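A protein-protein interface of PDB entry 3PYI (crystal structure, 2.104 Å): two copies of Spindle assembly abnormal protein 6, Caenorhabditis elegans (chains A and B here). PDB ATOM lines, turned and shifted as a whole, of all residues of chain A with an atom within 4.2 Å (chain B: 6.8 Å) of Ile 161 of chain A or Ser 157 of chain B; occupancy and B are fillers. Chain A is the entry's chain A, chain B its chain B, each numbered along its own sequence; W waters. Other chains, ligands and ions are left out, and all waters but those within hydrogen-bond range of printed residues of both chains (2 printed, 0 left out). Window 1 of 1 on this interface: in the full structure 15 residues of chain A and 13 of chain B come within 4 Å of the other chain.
NZ of Lys 158 of chain B is in salt-bridge range of OD1 of Asp 84 of chain A.
N of Ser 157 of chain B lies within hydrogen-bond range of OG1 of Thr 86 of chain A, at 3.2 Å.
The backbone NH (N) of Thr 86 of chain A lies within hydrogen-bond range of the backbone carbonyl oxygen (O) of Ile 156 of chain B (2.7 Å).
The side-chain hydroxyl (OG1) of Thr 154 of chain B sits at hydrogen-bond distance from the side-chain hydroxyl (OG) of Ser 157 of chain B (2.6 Å).
The backbone NH (N) of Leu 150 of chain A is in hydrogen-bond range of the backbone carbonyl oxygen (O) of Phe 162 of chain A, 3.0 Å away.
The backbone carbonyl oxygen of Leu 150 of chain A sits at hydrogen-bond distance from the backbone NH of Ile 161 of chain A.
OG1 of Thr 154 of chain B lies within hydrogen-bond range of N of Ile 156 of chain B (3.0 Å).
Ser 157 of chain B touches His 83 of chain A.
CA of Ser 157 of chain B touches O of Asp 84 of chain A (3.2 Å).
Leu 85 of chain A touches Ile 156 of chain B.
Ser 157 of chain B touches Leu 85 of chain A (CB to CD2, 3.9 Å).
Lys 158 of chain B touches Thr 86 of chain A (CG to CG2, 3.8 Å).
CD1 of Leu 100 of chain A touches CD1 of Ile 156 of chain B, at 3.9 Å.
Ile 156 of chain B touches Ile 161 of chain A (CG1 to CG2, 3.4 Å).
CG2 of Ile 161 of chain A touches OG of Ser 157 of chain B, at 3.7 Å.
Ile 156 of chain B touches Phe 162 of chain A.
Printed residues of chain B within 4 Å of His 83 of chain A: Ser 157 (3.99 Å).
Printed residues of chain B within 4 Å of Thr 86 of chain A: Ile 156, Ser 157 and Lys 158.
Of the printed residues of chain B, Leu 100 of chain A touches Ile 156.
Ser 152 of chain A touches none of the printed residues of chain B.
Of chain B, only Ile 156 (3.4 Å) and Ser 157 (3.7 Å) come within 4 Å of Ile 161 of chain A.
Of the printed residues of chain B, Phe 162 of chain A touches Ile 156.
Printed residues of chain A within 4 Å of Ser 157 of chain B: His 83, Asp 84, Leu 85, Thr 86 and Ile 161.
The nearest residue of chain B that does not touch Ile 161 of chain A is Thr 154 of chain B (4.2 Å).
The nearest printed residue of chain B that does not touch Thr 86 of chain A is Lys 153 of chain B (4.1 Å).
Hydrophobic or aromatic side chains of chain B within 4 Å of the printed part of chain A: Ile 156.
Among the printed residues, Asp or Glu carboxylates within 4 Å of a Lys or Arg side-chain nitrogen of the other chain: Asp 84 of chain A with Lys 158 of chain B.
Positions printed for both chains: 152, 159 and 160.
Of the 12 pairs that touch across the chains among the printed residues, none has its exchanged pair printed and touching as well.
Water W1 lies within hydrogen-bond range of the side-chain hydroxyl of Thr 86 of chain A (2.6 Å), the backbone carbonyl oxygen of Thr 154 of chain B (2.8 Å), the side-chain amino group of Lys 153 of chain B (3.1 Å) and the backbone carbonyl oxygen of Ser 157 of chain B (3.2 Å).
Water W2 lies within hydrogen-bond range of the backbone NH (N) of Lys 160 of chain B (2.9 Å), the side-chain carboxylate (OD2) of Asp 84 of chain A (3.1 Å) and the backbone NH (N) of Gly 159 of chain B (3.2 Å).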
ATOM      1  N   HIS A  83      -3.809 -10.212  -3.535  1.00  0.00           N
ATOM      2  CA  HIS A  83      -2.971 -11.227  -4.153  1.00  0.00           C
ATOM      3  C   HIS A  83      -1.879 -10.684  -5.059  1.00  0.00           C
ATOM      4  O   HIS A  83      -1.310 -11.444  -5.840  1.00  0.00           O
ATOM      5  CB  HIS A  83      -3.829 -12.224  -4.935  1.00  0.00           C
ATOM      6  CG  HIS A  83      -4.793 -12.978  -4.083  1.00  0.00           C
ATOM      7  ND1 HIS A  83      -6.128 -12.643  -3.995  1.00  0.00           N
ATOM      8  CD2 HIS A  83      -4.617 -14.044  -3.268  1.00  0.00           C
ATOM      9  CE1 HIS A  83      -6.734 -13.479  -3.171  1.00  0.00           C
ATOM     10  NE2 HIS A  83      -5.840 -14.339  -2.717  1.00  0.00           N
ATOM     11  N   ASP A  84      -1.588  -9.387  -4.967  1.00  0.00           N
ATOM     12  CA  ASP A  84      -0.542  -8.801  -5.807  1.00  0.00           C
ATOM     13  C   ASP A  84      -0.790  -9.072  -7.273  1.00  0.00           C
ATOM     14  O   ASP A  84       0.134  -9.406  -8.013  1.00  0.00           O
ATOM     15  CB  ASP A  84       0.833  -9.385  -5.445  1.00  0.00           C
ATOM     16  CG  ASP A  84       1.448  -8.737  -4.220  1.00  0.00           C
ATOM     17  OD1 ASP A  84       1.033  -7.617  -3.861  1.00  0.00           O
ATOM     18  OD2 ASP A  84       2.364  -9.349  -3.625  1.00  0.00           O
ATOM     19  N   LEU A  85      -2.037  -8.938  -7.710  1.00  0.00           N
ATOM     20  CA  LEU A  85      -2.328  -9.154  -9.116  1.00  0.00           C
ATOM     21  C   LEU A  85      -1.801  -7.967  -9.916  1.00  0.00           C
ATOM     22  O   LEU A  85      -1.826  -6.836  -9.440  1.00  0.00           O
ATOM     23  CB  LEU A  85      -3.829  -9.359  -9.343  1.00  0.00           C
ATOM     24  CG  LEU A  85      -4.445 -10.532  -8.574  1.00  0.00           C
ATOM     25  CD1 LEU A  85      -5.881 -10.792  -9.088  1.00  0.00           C
ATOM     26  CD2 LEU A  85      -3.584 -11.805  -8.682  1.00  0.00           C
ATOM     27  N   THR A  86      -1.308  -8.235 -11.118  1.00  0.00           N
ATOM     28  CA  THR A  86      -0.618  -7.216 -11.890  1.00  0.00           C
ATOM     29  C   THR A  86      -1.402  -6.788 -13.132  1.00  0.00           C
ATOM     30  O   THR A  86      -0.948  -5.942 -13.880  1.00  0.00           O
ATOM     31  CB  THR A  86       0.781  -7.699 -12.318  1.00  0.00           C
ATOM     32  OG1 THR A  86       0.685  -8.996 -12.930  1.00  0.00           O
ATOM     33  CG2 THR A  86       1.716  -7.766 -11.113  1.00  0.00           C
ATOM     34  N   LEU A 100      -3.504 -19.454 -18.286  1.00  0.00           N
ATOM     35  CA  LEU A 100      -3.510 -20.239 -17.058  1.00  0.00           C
ATOM     36  C   LEU A 100      -4.463 -21.442 -17.044  1.00  0.00           C
ATOM     37  O   LEU A 100      -4.083 -22.515 -16.592  1.00  0.00           O
ATOM     38  CB  LEU A 100      -3.792 -19.342 -15.844  1.00  0.00           C
ATOM     39  CG  LEU A 100      -2.748 -18.289 -15.456  1.00  0.00           C
ATOM     40  CD1 LEU A 100      -3.218 -17.527 -14.243  1.00  0.00           C
ATOM     41  CD2 LEU A 100      -1.397 -18.933 -15.169  1.00  0.00           C
ATOM     42  N   LEU A 150      -6.279 -20.897  -7.574  1.00  0.00           N
ATOM     43  CA  LEU A 150      -5.439 -21.207  -8.721  1.00  0.00           C
ATOM     44  C   LEU A 150      -3.958 -21.170  -8.303  1.00  0.00           C
ATOM     45  O   LEU A 150      -3.538 -20.264  -7.595  1.00  0.00           O
ATOM     46  CB  LEU A 150      -5.698 -20.166  -9.806  1.00  0.00           C
ATOM     47  CG  LEU A 150      -5.405 -20.523 -11.254  1.00  0.00           C
ATOM     48  CD1 LEU A 150      -6.090 -21.831 -11.603  1.00  0.00           C
ATOM     49  CD2 LEU A 150      -5.886 -19.398 -12.163  1.00  0.00           C
ATOM     50  N   SER A 152       0.310 -21.852  -9.520  1.00  0.00           N
ATOM     51  CA  SER A 152       1.352 -22.134 -10.492  1.00  0.00           C
ATOM     52  C   SER A 152       2.631 -22.486  -9.728  1.00  0.00           C
ATOM     53  O   SER A 152       3.345 -21.615  -9.232  1.00  0.00           O
ATOM     54  CB  SER A 152       1.572 -20.945 -11.428  1.00  0.00           C
ATOM     55  OG  SER A 152       2.498 -21.282 -12.438  1.00  0.00           O
ATOM     56  N   GLY A 159       3.075 -21.786  -5.038  1.00  0.00           N
ATOM     57  CA  GLY A 159       2.748 -20.774  -6.043  1.00  0.00           C
ATOM     58  C   GLY A 159       1.262 -20.446  -6.197  1.00  0.00           C
ATOM     59  O   GLY A 159       0.748 -20.354  -7.308  1.00  0.00           O
ATOM     60  N   LYS A 160       0.575 -20.268  -5.075  1.00  0.00           N
ATOM     61  CA  LYS A 160      -0.804 -19.814  -5.095  1.00  0.00           C
ATOM     62  C   LYS A 160      -0.887 -18.469  -5.802  1.00  0.00           C
ATOM     63  O   LYS A 160      -0.160 -17.536  -5.461  1.00  0.00           O
ATOM     64  CB  LYS A 160      -1.334 -19.678  -3.667  1.00  0.00           C
ATOM     65  CG  LYS A 160      -2.805 -19.272  -3.582  1.00  0.00           C
ATOM     66  CD  LYS A 160      -3.333 -19.543  -2.179  1.00  0.00           C
ATOM     67  CE  LYS A 160      -4.517 -18.662  -1.841  1.00  0.00           C
ATOM     68  NZ  LYS A 160      -4.999 -18.918  -0.457  1.00  0.00           N
ATOM     69  N   ILE A 161      -1.762 -18.367  -6.793  1.00  0.00           N
ATOM     70  CA  ILE A 161      -1.949 -17.087  -7.469  1.00  0.00           C
ATOM     71  C   ILE A 161      -3.074 -16.263  -6.858  1.00  0.00           C
ATOM     72  O   ILE A 161      -2.876 -15.098  -6.510  1.00  0.00           O
ATOM     73  CB  ILE A 161      -2.178 -17.242  -8.970  1.00  0.00           C
ATOM     74  CG1 ILE A 161      -1.034 -18.040  -9.584  1.00  0.00           C
ATOM     75  CG2 ILE A 161      -2.280 -15.869  -9.624  1.00  0.00           C
ATOM     76  CD1 ILE A 161      -1.118 -18.149 -11.074  1.00  0.00           C
ATOM     77  N   PHE A 162      -4.255 -16.852  -6.735  1.00  0.00           N
ATOM     78  CA  PHE A 162      -5.350 -16.159  -6.060  1.00  0.00           C
ATOM     79  C   PHE A 162      -6.363 -17.165  -5.562  1.00  0.00           C
ATOM     80  O   PHE A 162      -6.329 -18.330  -5.945  1.00  0.00           O
ATOM     81  CB  PHE A 162      -6.033 -15.138  -6.990  1.00  0.00           C
ATOM     82  CG  PHE A 162      -6.755 -15.757  -8.151  1.00  0.00           C
ATOM     83  CD1 PHE A 162      -6.199 -15.746  -9.416  1.00  0.00           C
ATOM     84  CD2 PHE A 162      -7.998 -16.344  -7.976  1.00  0.00           C
ATOM     85  CE1 PHE A 162      -6.863 -16.315 -10.490  1.00  0.00           C
ATOM     86  CE2 PHE A 162      -8.667 -16.921  -9.038  1.00  0.00           C
ATOM     87  CZ  PHE A 162      -8.105 -16.906 -10.299  1.00  0.00           C
ATOM     88  N   LYS B 131       8.380 -16.894 -15.038  1.00  0.00           N
ATOM     89  CA  LYS B 131       9.277 -15.968 -15.716  1.00  0.00           C
ATOM     90  C   LYS B 131      10.544 -15.794 -14.888  1.00  0.00           C
ATOM     91  O   LYS B 131      10.592 -16.221 -13.735  1.00  0.00           O
ATOM     92  CB  LYS B 131       8.584 -14.615 -15.905  1.00  0.00           C
ATOM     93  CG  LYS B 131       7.198 -14.706 -16.535  1.00  0.00           C
ATOM     94  CD  LYS B 131       6.509 -13.351 -16.570  1.00  0.00           C
ATOM     95  CE  LYS B 131       5.090 -13.472 -17.101  1.00  0.00           C
ATOM     96  NZ  LYS B 131       4.392 -12.156 -17.135  1.00  0.00           N
ATOM     97  N   SER B 152       8.961 -14.848  -8.457  1.00  0.00           N
ATOM     98  CA  SER B 152       8.898 -15.466  -9.772  1.00  0.00           C
ATOM     99  C   SER B 152       7.562 -15.095 -10.424  1.00  0.00           C
ATOM    100  O   SER B 152       6.526 -15.670 -10.112  1.00  0.00           O
ATOM    101  CB  SER B 152       9.077 -16.987  -9.643  1.00  0.00           C
ATOM    102  OG  SER B 152       9.110 -17.603 -10.914  1.00  0.00           O
ATOM    103  N   LYS B 153       7.600 -14.120 -11.317  1.00  0.00           N
ATOM    104  CA  LYS B 153       6.396 -13.488 -11.868  1.00  0.00           C
ATOM    105  C   LYS B 153       5.448 -14.476 -12.542  1.00  0.00           C
ATOM    106  O   LYS B 153       5.895 -15.417 -13.187  1.00  0.00           O
ATOM    107  CB  LYS B 153       6.830 -12.425 -12.878  1.00  0.00           C
ATOM    108  CG  LYS B 153       5.833 -11.328 -13.159  1.00  0.00           C
ATOM    109  CD  LYS B 153       6.447 -10.305 -14.119  1.00  0.00           C
ATOM    110  CE  LYS B 153       5.569  -9.070 -14.271  1.00  0.00           C
ATOM    111  NZ  LYS B 153       5.282  -8.424 -12.958  1.00  0.00           N
ATOM    112  N   THR B 154       4.141 -14.274 -12.391  1.00  0.00           N
ATOM    113  CA  THR B 154       3.175 -15.067 -13.159  1.00  0.00           C
ATOM    114  C   THR B 154       2.514 -14.131 -14.164  1.00  0.00           C
ATOM    115  O   THR B 154       2.754 -12.930 -14.125  1.00  0.00           O
ATOM    116  CB  THR B 154       2.085 -15.697 -12.283  1.00  0.00           C
ATOM    117  OG1 THR B 154       1.055 -14.732 -12.051  1.00  0.00           O
ATOM    118  CG2 THR B 154       2.668 -16.206 -10.948  1.00  0.00           C
ATOM    119  N   PRO B 155       1.686 -14.676 -15.068  1.00  0.00           N
ATOM    120  CA  PRO B 155       0.999 -13.782 -16.006  1.00  0.00           C
ATOM    121  C   PRO B 155       0.030 -12.811 -15.333  1.00  0.00           C
ATOM    122  O   PRO B 155      -0.333 -11.834 -15.971  1.00  0.00           O
ATOM    123  CB  PRO B 155       0.243 -14.747 -16.923  1.00  0.00           C
ATOM    124  CG  PRO B 155       1.029 -16.030 -16.839  1.00  0.00           C
ATOM    125  CD  PRO B 155       1.530 -16.099 -15.433  1.00  0.00           C
ATOM    126  N   ILE B 156      -0.396 -13.055 -14.097  1.00  0.00           N
ATOM    127  CA  ILE B 156      -1.366 -12.143 -13.485  1.00  0.00           C
ATOM    128  C   ILE B 156      -0.940 -11.593 -12.139  1.00  0.00           C
ATOM    129  O   ILE B 156      -1.703 -10.872 -11.496  1.00  0.00           O
ATOM    130  CB  ILE B 156      -2.785 -12.772 -13.319  1.00  0.00           C
ATOM    131  CG1 ILE B 156      -2.770 -13.966 -12.371  1.00  0.00           C
ATOM    132  CG2 ILE B 156      -3.357 -13.175 -14.655  1.00  0.00           C
ATOM    133  CD1 ILE B 156      -4.185 -14.473 -12.078  1.00  0.00           C
ATOM    134  N   SER B 157       0.273 -11.922 -11.711  1.00  0.00           N
ATOM    135  CA  SER B 157       0.672 -11.583 -10.354  1.00  0.00           C
ATOM    136  C   SER B 157       2.184 -11.495 -10.180  1.00  0.00           C
ATOM    137  O   SER B 157       2.965 -11.979 -11.007  1.00  0.00           O
ATOM    138  CB  SER B 157       0.130 -12.626  -9.372  1.00  0.00           C
ATOM    139  OG  SER B 157       0.793 -13.855  -9.581  1.00  0.00           O
ATOM    140  N   LYS B 158       2.585 -10.906  -9.062  1.00  0.00           N
ATOM    141  CA  LYS B 158       3.996 -10.670  -8.775  1.00  0.00           C
ATOM    142  C   LYS B 158       4.767 -11.959  -8.499  1.00  0.00           C
ATOM    143  O   LYS B 158       5.954 -12.042  -8.807  1.00  0.00           O
ATOM    144  CB  LYS B 158       4.134  -9.699  -7.602  1.00  0.00           C
ATOM    145  CG  LYS B 158       3.674  -8.263  -7.940  1.00  0.00           C
ATOM    146  CD  LYS B 158       3.701  -7.383  -6.704  1.00  0.00           C
ATOM    147  CE  LYS B 158       3.537  -5.908  -7.059  1.00  0.00           C
ATOM    148  NZ  LYS B 158       3.378  -5.056  -5.840  1.00  0.00           N
ATOM    149  N   GLY B 159       4.098 -12.953  -7.911  1.00  0.00           N
ATOM    150  CA  GLY B 159       4.730 -14.243  -7.638  1.00  0.00           C
ATOM    151  C   GLY B 159       5.798 -14.207  -6.547  1.00  0.00           C
ATOM    152  O   GLY B 159       6.861 -14.811  -6.670  1.00  0.00           O
ATOM    153  N   LYS B 160       5.519 -13.498  -5.463  1.00  0.00           N
ATOM    154  CA  LYS B 160       6.438 -13.473  -4.344  1.00  0.00           C
ATOM    155  C   LYS B 160       6.619 -14.895  -3.823  1.00  0.00           C
ATOM    156  O   LYS B 160       5.635 -15.607  -3.574  1.00  0.00           O
ATOM    157  CB  LYS B 160       5.895 -12.578  -3.237  1.00  0.00           C
ATOM    158  CG  LYS B 160       6.819 -12.461  -2.021  1.00  0.00           C
ATOM    159  CD  LYS B 160       6.381 -11.287  -1.153  1.00  0.00           C
ATOM    160  CE  LYS B 160       6.819 -11.454   0.287  1.00  0.00           C
ATOM    161  NZ  LYS B 160       6.354 -10.315   1.124  1.00  0.00           N
HETATM  162  O   HOH W   1       2.857 -10.191 -13.681  1.00  0.00           O
HETATM  163  O   HOH W   2       3.067 -12.078  -4.996  1.00  0.00           O
